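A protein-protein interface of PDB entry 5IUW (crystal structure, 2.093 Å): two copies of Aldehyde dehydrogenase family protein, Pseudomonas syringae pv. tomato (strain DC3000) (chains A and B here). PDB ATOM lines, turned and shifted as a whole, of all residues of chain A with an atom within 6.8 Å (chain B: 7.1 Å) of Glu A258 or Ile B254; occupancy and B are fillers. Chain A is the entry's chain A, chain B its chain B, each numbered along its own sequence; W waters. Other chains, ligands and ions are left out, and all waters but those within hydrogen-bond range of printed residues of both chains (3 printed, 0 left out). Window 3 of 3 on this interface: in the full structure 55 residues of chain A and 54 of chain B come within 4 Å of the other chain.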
ATOM      1  N   LYS A 229     -17.924  11.463  17.633  1.00  0.00           N
ATOM      2  CA  LYS A 229     -18.994  10.990  16.783  1.00  0.00           C
ATOM      3  C   LYS A 229     -20.204  11.912  16.876  1.00  0.00           C
ATOM      4  O   LYS A 229     -20.814  12.232  15.865  1.00  0.00           O
ATOM      5  CB  LYS A 229     -19.353   9.550  17.180  1.00  0.00           C
ATOM      6  CG  LYS A 229     -20.517   8.938  16.452  1.00  0.00           C
ATOM      7  CD  LYS A 229     -20.765   7.517  16.970  1.00  0.00           C
ATOM      8  CE  LYS A 229     -22.019   6.919  16.360  1.00  0.00           C
ATOM      9  NZ  LYS A 229     -22.185   5.481  16.730  1.00  0.00           N
ATOM     10  N   LEU A 233     -21.874  13.861  13.717  1.00  0.00           N
ATOM     11  CA  LEU A 233     -23.271  13.596  13.386  1.00  0.00           C
ATOM     12  C   LEU A 233     -24.198  14.777  13.679  1.00  0.00           C
ATOM     13  O   LEU A 233     -25.392  14.696  13.437  1.00  0.00           O
ATOM     14  CB  LEU A 233     -23.779  12.370  14.161  1.00  0.00           C
ATOM     15  CG  LEU A 233     -23.324  11.021  13.620  1.00  0.00           C
ATOM     16  CD1 LEU A 233     -23.643   9.914  14.634  1.00  0.00           C
ATOM     17  CD2 LEU A 233     -24.027  10.762  12.290  1.00  0.00           C
ATOM     18  N   MET A 235     -26.459  17.957  13.603  1.00  0.00           N
ATOM     19  CA  MET A 235     -27.198  18.546  12.497  1.00  0.00           C
ATOM     20  C   MET A 235     -26.966  20.051  12.358  1.00  0.00           C
ATOM     21  O   MET A 235     -27.393  20.654  11.379  1.00  0.00           O
ATOM     22  CB  MET A 235     -28.692  18.268  12.653  1.00  0.00           C
ATOM     23  CG  MET A 235     -29.043  16.799  12.583  1.00  0.00           C
ATOM     24  SD  MET A 235     -28.780  16.111  10.928  1.00  0.00           S
ATOM     25  CE  MET A 235     -30.042  16.898   9.946  1.00  0.00           C
ATOM     26  N   LYS A 250     -12.585   8.108   6.984  1.00  0.00           N
ATOM     27  CA  LYS A 250     -13.666   7.541   6.180  1.00  0.00           C
ATOM     28  C   LYS A 250     -14.998   7.534   6.915  1.00  0.00           C
ATOM     29  O   LYS A 250     -16.031   7.884   6.340  1.00  0.00           O
ATOM     30  CB  LYS A 250     -13.323   6.116   5.757  1.00  0.00           C
ATOM     31  CG  LYS A 250     -12.284   6.040   4.665  1.00  0.00           C
ATOM     32  CD  LYS A 250     -11.939   4.586   4.393  1.00  0.00           C
ATOM     33  CE  LYS A 250     -10.871   4.486   3.340  1.00  0.00           C
ATOM     34  NZ  LYS A 250     -10.275   3.135   3.259  1.00  0.00           N
ATOM     35  N   GLN A 251     -14.966   7.128   8.185  1.00  0.00           N
ATOM     36  CA  GLN A 251     -16.159   7.101   9.031  1.00  0.00           C
ATOM     37  C   GLN A 251     -16.810   8.464   9.122  1.00  0.00           C
ATOM     38  O   GLN A 251     -18.028   8.570   9.172  1.00  0.00           O
ATOM     39  CB  GLN A 251     -15.820   6.611  10.448  1.00  0.00           C
ATOM     40  CG  GLN A 251     -16.130   5.142  10.707  1.00  0.00           C
ATOM     41  CD  GLN A 251     -17.624   4.803  10.635  1.00  0.00           C
ATOM     42  OE1 GLN A 251     -18.484   5.684  10.575  1.00  0.00           O
ATOM     43  NE2 GLN A 251     -17.931   3.513  10.644  1.00  0.00           N
ATOM     44  N   MET A 253     -16.875  10.727   6.766  1.00  0.00           N
ATOM     45  CA  MET A 253     -17.640  10.964   5.537  1.00  0.00           C
ATOM     46  C   MET A 253     -19.001  10.310   5.669  1.00  0.00           C
ATOM     47  O   MET A 253     -20.025  10.879   5.299  1.00  0.00           O
ATOM     48  CB  MET A 253     -16.903  10.425   4.307  1.00  0.00           C
ATOM     49  CG  MET A 253     -15.546  11.096   4.074  1.00  0.00           C
ATOM     50  SD  MET A 253     -14.776  10.777   2.475  1.00  0.00           S
ATOM     51  CE  MET A 253     -15.871  11.720   1.401  1.00  0.00           C
ATOM     52  N   ILE A 254     -19.002   9.105   6.222  1.00  0.00           N
ATOM     53  CA  ILE A 254     -20.242   8.378   6.441  1.00  0.00           C
ATOM     54  C   ILE A 254     -21.161   9.166   7.387  1.00  0.00           C
ATOM     55  O   ILE A 254     -22.323   9.390   7.068  1.00  0.00           O
ATOM     56  CB  ILE A 254     -19.956   6.959   6.976  1.00  0.00           C
ATOM     57  CG1 ILE A 254     -19.332   6.112   5.862  1.00  0.00           C
ATOM     58  CG2 ILE A 254     -21.237   6.294   7.486  1.00  0.00           C
ATOM     59  CD1 ILE A 254     -18.773   4.768   6.332  1.00  0.00           C
ATOM     60  N   TYR A 255     -20.628   9.621   8.523  1.00  0.00           N
ATOM     61  CA  TYR A 255     -21.396  10.451   9.459  1.00  0.00           C
ATOM     62  C   TYR A 255     -22.012  11.685   8.814  1.00  0.00           C
ATOM     63  O   TYR A 255     -23.132  12.062   9.128  1.00  0.00           O
ATOM     64  CB  TYR A 255     -20.518  10.915  10.619  1.00  0.00           C
ATOM     65  CG  TYR A 255     -20.053   9.820  11.539  1.00  0.00           C
ATOM     66  CD1 TYR A 255     -20.811   8.677  11.731  1.00  0.00           C
ATOM     67  CD2 TYR A 255     -18.845   9.942  12.225  1.00  0.00           C
ATOM     68  CE1 TYR A 255     -20.374   7.678  12.584  1.00  0.00           C
ATOM     69  CE2 TYR A 255     -18.401   8.959  13.074  1.00  0.00           C
ATOM     70  CZ  TYR A 255     -19.163   7.830  13.257  1.00  0.00           C
ATOM     71  OH  TYR A 255     -18.708   6.859  14.105  1.00  0.00           O
ATOM     72  N   ALA A 256     -21.261  12.336   7.939  1.00  0.00           N
ATOM     73  CA  ALA A 256     -21.771  13.519   7.276  1.00  0.00           C
ATOM     74  C   ALA A 256     -22.916  13.159   6.329  1.00  0.00           C
ATOM     75  O   ALA A 256     -23.899  13.870   6.249  1.00  0.00           O
ATOM     76  CB  ALA A 256     -20.662  14.221   6.531  1.00  0.00           C
ATOM     77  N   GLY A 257     -22.792  12.039   5.631  1.00  0.00           N
ATOM     78  CA  GLY A 257     -23.858  11.591   4.756  1.00  0.00           C
ATOM     79  C   GLY A 257     -25.105  11.170   5.514  1.00  0.00           C
ATOM     80  O   GLY A 257     -26.210  11.344   5.020  1.00  0.00           O
ATOM     81  N   GLU A 258     -24.918  10.619   6.712  1.00  0.00           N
ATOM     82  CA  GLU A 258     -26.019  10.183   7.564  1.00  0.00           C
ATOM     83  C   GLU A 258     -26.745  11.338   8.227  1.00  0.00           C
ATOM     84  O   GLU A 258     -27.869  11.175   8.683  1.00  0.00           O
ATOM     85  CB  GLU A 258     -25.518   9.229   8.657  1.00  0.00           C
ATOM     86  CG  GLU A 258     -25.152   7.842   8.153  1.00  0.00           C
ATOM     87  CD  GLU A 258     -24.605   6.936   9.244  1.00  0.00           C
ATOM     88  OE1 GLU A 258     -24.393   7.409  10.378  1.00  0.00           O
ATOM     89  OE2 GLU A 258     -24.377   5.745   8.964  1.00  0.00           O
ATOM     90  N   SER A 259     -26.103  12.501   8.304  1.00  0.00           N
ATOM     91  CA  SER A 259     -26.685  13.591   9.062  1.00  0.00           C
ATOM     92  C   SER A 259     -27.069  14.744   8.150  1.00  0.00           C
ATOM     93  O   SER A 259     -28.121  14.711   7.533  1.00  0.00           O
ATOM     94  CB  SER A 259     -25.730  14.061  10.178  1.00  0.00           C
ATOM     95  OG  SER A 259     -24.468  14.462   9.679  1.00  0.00           O
ATOM     96  N   ASN A 260     -26.218  15.761   8.050  1.00  0.00           N
ATOM     97  CA  ASN A 260     -26.635  16.989   7.389  1.00  0.00           C
ATOM     98  C   ASN A 260     -25.775  17.441   6.213  1.00  0.00           C
ATOM     99  O   ASN A 260     -25.800  18.623   5.874  1.00  0.00           O
ATOM    100  CB  ASN A 260     -26.683  18.129   8.417  1.00  0.00           C
ATOM    101  CG  ASN A 260     -25.281  18.576   8.881  1.00  0.00           C
ATOM    102  OD1 ASN A 260     -24.292  17.841   8.751  1.00  0.00           O
ATOM    103  ND2 ASN A 260     -25.207  19.788   9.430  1.00  0.00           N
ATOM    104  N   MET A 261     -25.013  16.524   5.615  1.00  0.00           N
ATOM    105  CA  MET A 261     -24.153  16.860   4.475  1.00  0.00           C
ATOM    106  C   MET A 261     -23.132  17.945   4.831  1.00  0.00           C
ATOM    107  O   MET A 261     -22.764  18.744   3.978  1.00  0.00           O
ATOM    108  CB  MET A 261     -25.003  17.320   3.271  1.00  0.00           C
ATOM    109  CG  MET A 261     -24.329  17.230   1.899  1.00  0.00           C
ATOM    110  SD  MET A 261     -25.332  17.975   0.568  1.00  0.00           S
ATOM    111  CE  MET A 261     -26.751  16.921   0.692  1.00  0.00           C
ATOM    112  N   ALA B 232     -19.688   5.435  -7.825  1.00  0.00           N
ATOM    113  CA  ALA B 232     -19.493   6.111  -6.547  1.00  0.00           C
ATOM    114  C   ALA B 232     -18.762   5.229  -5.533  1.00  0.00           C
ATOM    115  O   ALA B 232     -18.068   5.734  -4.662  1.00  0.00           O
ATOM    116  CB  ALA B 232     -20.827   6.561  -5.991  1.00  0.00           C
ATOM    117  N   LEU B 233     -18.901   3.914  -5.663  1.00  0.00           N
ATOM    118  CA  LEU B 233     -18.205   2.979  -4.784  1.00  0.00           C
ATOM    119  C   LEU B 233     -16.890   2.460  -5.361  1.00  0.00           C
ATOM    120  O   LEU B 233     -16.241   1.615  -4.755  1.00  0.00           O
ATOM    121  CB  LEU B 233     -19.103   1.780  -4.467  1.00  0.00           C
ATOM    122  CG  LEU B 233     -20.203   1.959  -3.432  1.00  0.00           C
ATOM    123  CD1 LEU B 233     -21.200   0.832  -3.540  1.00  0.00           C
ATOM    124  CD2 LEU B 233     -19.587   2.006  -2.012  1.00  0.00           C
ATOM    125  N   ILE B 248     -29.869  11.780  -2.512  1.00  0.00           N
ATOM    126  CA  ILE B 248     -28.858  10.963  -3.169  1.00  0.00           C
ATOM    127  C   ILE B 248     -27.460  11.552  -2.975  1.00  0.00           C
ATOM    128  O   ILE B 248     -26.474  10.820  -2.880  1.00  0.00           O
ATOM    129  CB  ILE B 248     -29.148  10.810  -4.674  1.00  0.00           C
ATOM    130  CG1 ILE B 248     -30.491  10.109  -4.889  1.00  0.00           C
ATOM    131  CG2 ILE B 248     -28.056   9.998  -5.351  1.00  0.00           C
ATOM    132  CD1 ILE B 248     -30.487   8.663  -4.445  1.00  0.00           C
ATOM    133  N   ALA B 249     -27.385  12.877  -2.911  1.00  0.00           N
ATOM    134  CA  ALA B 249     -26.117  13.543  -2.639  1.00  0.00           C
ATOM    135  C   ALA B 249     -25.493  13.045  -1.334  1.00  0.00           C
ATOM    136  O   ALA B 249     -24.302  12.753  -1.287  1.00  0.00           O
ATOM    137  CB  ALA B 249     -26.305  15.054  -2.598  1.00  0.00           C
ATOM    138  N   LYS B 250     -26.302  12.934  -0.287  1.00  0.00           N
ATOM    139  CA  LYS B 250     -25.839  12.401   0.997  1.00  0.00           C
ATOM    140  C   LYS B 250     -25.335  10.961   0.891  1.00  0.00           C
ATOM    141  O   LYS B 250     -24.335  10.599   1.523  1.00  0.00           O
ATOM    142  CB  LYS B 250     -26.954  12.461   2.042  1.00  0.00           C
ATOM    143  CG  LYS B 250     -27.193  13.840   2.622  1.00  0.00           C
ATOM    144  CD  LYS B 250     -28.564  13.911   3.282  1.00  0.00           C
ATOM    145  CE  LYS B 250     -28.698  15.164   4.106  1.00  0.00           C
ATOM    146  NZ  LYS B 250     -30.037  15.295   4.723  1.00  0.00           N
ATOM    147  N   GLN B 251     -26.031  10.147   0.098  1.00  0.00           N
ATOM    148  CA  GLN B 251     -25.626   8.760  -0.119  1.00  0.00           C
ATOM    149  C   GLN B 251     -24.238   8.660  -0.738  1.00  0.00           C
ATOM    150  O   GLN B 251     -23.517   7.704  -0.483  1.00  0.00           O
ATOM    151  CB  GLN B 251     -26.625   8.025  -1.023  1.00  0.00           C
ATOM    152  CG  GLN B 251     -27.686   7.223  -0.294  1.00  0.00           C
ATOM    153  CD  GLN B 251     -27.116   6.076   0.547  1.00  0.00           C
ATOM    154  OE1 GLN B 251     -26.066   5.513   0.237  1.00  0.00           O
ATOM    155  NE2 GLN B 251     -27.827   5.725   1.614  1.00  0.00           N
ATOM    156  N   LEU B 252     -23.878   9.631  -1.574  1.00  0.00           N
ATOM    157  CA  LEU B 252     -22.563   9.609  -2.211  1.00  0.00           C
ATOM    158  C   LEU B 252     -21.447   9.795  -1.177  1.00  0.00           C
ATOM    159  O   LEU B 252     -20.389   9.178  -1.282  1.00  0.00           O
ATOM    160  CB  LEU B 252     -22.454  10.675  -3.306  1.00  0.00           C
ATOM    161  CG  LEU B 252     -23.401  10.594  -4.513  1.00  0.00           C
ATOM    162  CD1 LEU B 252     -22.827  11.356  -5.697  1.00  0.00           C
ATOM    163  CD2 LEU B 252     -23.693   9.167  -4.907  1.00  0.00           C
ATOM    164  N   MET B 253     -21.687  10.649  -0.191  1.00  0.00           N
ATOM    165  CA  MET B 253     -20.735  10.827   0.899  1.00  0.00           C
ATOM    166  C   MET B 253     -20.534   9.498   1.617  1.00  0.00           C
ATOM    167  O   MET B 253     -19.409   9.104   1.927  1.00  0.00           O
ATOM    168  CB  MET B 253     -21.219  11.904   1.863  1.00  0.00           C
ATOM    169  CG  MET B 253     -21.283  13.274   1.207  1.00  0.00           C
ATOM    170  SD  MET B 253     -21.411  14.640   2.362  1.00  0.00           S
ATOM    171  CE  MET B 253     -19.719  14.657   2.996  1.00  0.00           C
ATOM    172  N   ILE B 254     -21.632   8.786   1.827  1.00  0.00           N
ATOM    173  CA  ILE B 254     -21.568   7.503   2.504  1.00  0.00           C
ATOM    174  C   ILE B 254     -20.759   6.503   1.664  1.00  0.00           C
ATOM    175  O   ILE B 254     -19.842   5.879   2.189  1.00  0.00           O
ATOM    176  CB  ILE B 254     -22.985   6.974   2.817  1.00  0.00           C
ATOM    177  CG1 ILE B 254     -23.643   7.838   3.899  1.00  0.00           C
ATOM    178  CG2 ILE B 254     -22.945   5.512   3.223  1.00  0.00           C
ATOM    179  CD1 ILE B 254     -25.091   7.497   4.194  1.00  0.00           C
ATOM    180  N   TYR B 255     -21.069   6.392   0.368  1.00  0.00           N
ATOM    181  CA  TYR B 255     -20.311   5.516  -0.536  1.00  0.00           C
ATOM    182  C   TYR B 255     -18.820   5.843  -0.551  1.00  0.00           C
ATOM    183  O   TYR B 255     -17.994   4.943  -0.626  1.00  0.00           O
ATOM    184  CB  TYR B 255     -20.818   5.597  -1.985  1.00  0.00           C
ATOM    185  CG  TYR B 255     -22.246   5.190  -2.240  1.00  0.00           C
ATOM    186  CD1 TYR B 255     -22.839   4.151  -1.541  1.00  0.00           C
ATOM    187  CD2 TYR B 255     -22.999   5.842  -3.215  1.00  0.00           C
ATOM    188  CE1 TYR B 255     -24.146   3.783  -1.792  1.00  0.00           C
ATOM    189  CE2 TYR B 255     -24.309   5.482  -3.473  1.00  0.00           C
ATOM    190  CZ  TYR B 255     -24.875   4.450  -2.753  1.00  0.00           C
ATOM    191  OH  TYR B 255     -26.171   4.084  -2.994  1.00  0.00           O
ATOM    192  N   ALA B 256     -18.472   7.128  -0.523  1.00  0.00           N
ATOM    193  CA  ALA B 256     -17.061   7.491  -0.534  1.00  0.00           C
ATOM    194  C   ALA B 256     -16.372   6.972   0.721  1.00  0.00           C
ATOM    195  O   ALA B 256     -15.254   6.454   0.661  1.00  0.00           O
ATOM    196  CB  ALA B 256     -16.888   8.985  -0.650  1.00  0.00           C
ATOM    197  N   GLY B 257     -17.057   7.111   1.855  1.00  0.00           N
ATOM    198  CA  GLY B 257     -16.547   6.612   3.117  1.00  0.00           C
ATOM    199  C   GLY B 257     -16.427   5.098   3.139  1.00  0.00           C
ATOM    200  O   GLY B 257     -15.528   4.558   3.766  1.00  0.00           O
ATOM    201  N   GLU B 258     -17.336   4.411   2.452  1.00  0.00           N
ATOM    202  CA  GLU B 258     -17.320   2.948   2.423  1.00  0.00           C
ATOM    203  C   GLU B 258     -16.260   2.422   1.467  1.00  0.00           C
ATOM    204  O   GLU B 258     -15.859   1.271   1.548  1.00  0.00           O
ATOM    205  CB  GLU B 258     -18.688   2.388   2.011  1.00  0.00           C
ATOM    206  CG  GLU B 258     -19.816   2.643   3.002  1.00  0.00           C
ATOM    207  CD  GLU B 258     -21.158   2.120   2.493  1.00  0.00           C
ATOM    208  OE1 GLU B 258     -21.278   1.835   1.283  1.00  0.00           O
ATOM    209  OE2 GLU B 258     -22.091   1.985   3.303  1.00  0.00           O
ATOM    210  N   SER B 259     -15.812   3.262   0.546  1.00  0.00           N
ATOM    211  CA  SER B 259     -14.882   2.787  -0.458  1.00  0.00           C
ATOM    212  C   SER B 259     -13.490   3.357  -0.255  1.00  0.00           C
ATOM    213  O   SER B 259     -12.716   2.828   0.530  1.00  0.00           O
ATOM    214  CB  SER B 259     -15.406   3.100  -1.880  1.00  0.00           C
ATOM    215  OG  SER B 259     -15.781   4.466  -2.031  1.00  0.00           O
ATOM    216  N   VAL B 264     -15.681  14.167  -2.899  1.00  0.00           N
ATOM    217  CA  VAL B 264     -17.091  14.227  -3.260  1.00  0.00           C
ATOM    218  C   VAL B 264     -17.550  15.675  -3.378  1.00  0.00           C
ATOM    219  O   VAL B 264     -17.444  16.436  -2.428  1.00  0.00           O
ATOM    220  CB  VAL B 264     -17.959  13.484  -2.219  1.00  0.00           C
ATOM    221  CG1 VAL B 264     -19.459  13.639  -2.521  1.00  0.00           C
ATOM    222  CG2 VAL B 264     -17.571  12.025  -2.184  1.00  0.00           C
HETATM  223  O   HOH W   1     -20.297  18.148   2.018  1.00  0.00           O
HETATM  224  O   HOH W   2     -30.277  13.197   6.522  1.00  0.00           O
HETATM  225  O   HOH W   3     -12.265   1.170   2.858  1.00  0.00           O
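Lys A250 touches Gly B257, and with the chains exchanged Gly A257 touches Lys B250. Lys A250 touches Ser B259, and with the chains exchanged Ser A259 touches Lys B250. Gly A257 touches Met B253, but with the chains exchanged Met A253 does not touch Gly B257 (4.01 Å). Glu A258 touches Ile B254, but with the chains exchanged Ile A254 does not touch Glu B258 (4.1 Å).
Hydrophobic or aromatic side chains of chain B within 4 Å of the printed part of chain A: Ala B249, Met B253, Ile B254, Ala B256 and Val B264. Hydrophobic or aromatic side chains of chain A within 4 Å of the printed part of chain B: Met A253, Ile A254, Ala A256 and Met A261. Along chain A the printed residues that touch a printed residue of chain B span positions 250 to 261. Among the printed residues, 16 pairs touch across the chains. Among the printed residues, no Asp or Glu carboxylate lies within 4 Å of a Lys or Arg side-chain nitrogen of the other chain.
Glu A258 touches one residue of chain B. Ile B254 touches just these residues of chain A: Ile A254, Gly A257 and Glu A258. Gly A257 touches three residues of chain B. Of the printed residues of chain A, Ser B259 touches Lys A250 (3.7 Å). Of the printed residues of chain A, Gly B257 touches Lys A250 and Ile A254. Printed residues of chain B within 4 Å of Ala A256: Met B253. Of the printed residues of chain A, Lys B250 touches Gly A257 (3.3 Å), Ser A259 (3.5 Å) and Met A261 (3.7 Å). Gln A251 touches none of the printed residues of chain B. Glu B258 touches none of the printed residues of chain A. The nearest residue of chain B that does not touch Glu A258 is Lys B250 (5.2 Å). The nearest printed residue of chain A that does not touch Met B253 is Ile A254 (4.3 Å).
Water W2 bridges the side-chain amino group (NZ) of Lys B250 (2.8 Å) and the backbone carbonyl oxygen (O) of Ser A259 (2.8 Å). Water W3 lies within hydrogen-bond range of the side-chain amino group of Lys A250 (2.8 Å) and the backbone carbonyl oxygen of Ser B259 (2.9 Å). Water W1 bridges the backbone carbonyl oxygen of Met A261 (3.2 Å) and the side-chain sulfur of Met B253 (3.7 Å).
Among the printed residues, pairs that only touch across the chains: Gly A257 with Lys B250 (3.3 Å), Lys A250 with Gly B257 (3.4 Å), Met A253 with Ala B256 (3.6 Å), Met A261 with Lys B250 (3.7 Å), Lys A250 with Ser B259 (3.7 Å), Ala A256 with Met B253 (3.7 Å), Met A253 with Met B253 (3.7 Å), Ile A254 with Ile B254 (3.7 Å), Met A261 with Ala B249 (3.8 Å), Gly A257 with Ile B254 (3.9 Å), Gly A257 with Met B253 (3.9 Å), Met A261 with Met B253 (3.9 Å), Ile A254 with Gly B257 (3.9 Å), Glu A258 with Ile B254 (3.97 Å) and Met A253 with Val B264 (3.98 Å).
The side-chain hydroxyl of Ser A259 lies within hydrogen-bond range of the backbone carbonyl oxygen of Tyr A255 (2.8 Å). The backbone NH (N) of Met A261 is in hydrogen-bond range of the backbone carbonyl oxygen (O) of Ala A256 (2.9 Å). O of Tyr B255 lies within hydrogen-bond range of OG of Ser B259 (2.7 Å). The side-chain hydroxyl (OG) of Ser B259 lies within hydrogen-bond range of the backbone carbonyl oxygen (O) of Ala B256, at 3.4 Å.
The side-chain amino group (NZ) of Lys B250 lies within hydrogen-bond range of the backbone carbonyl oxygen (O) of Ser A259 (3.5 Å).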
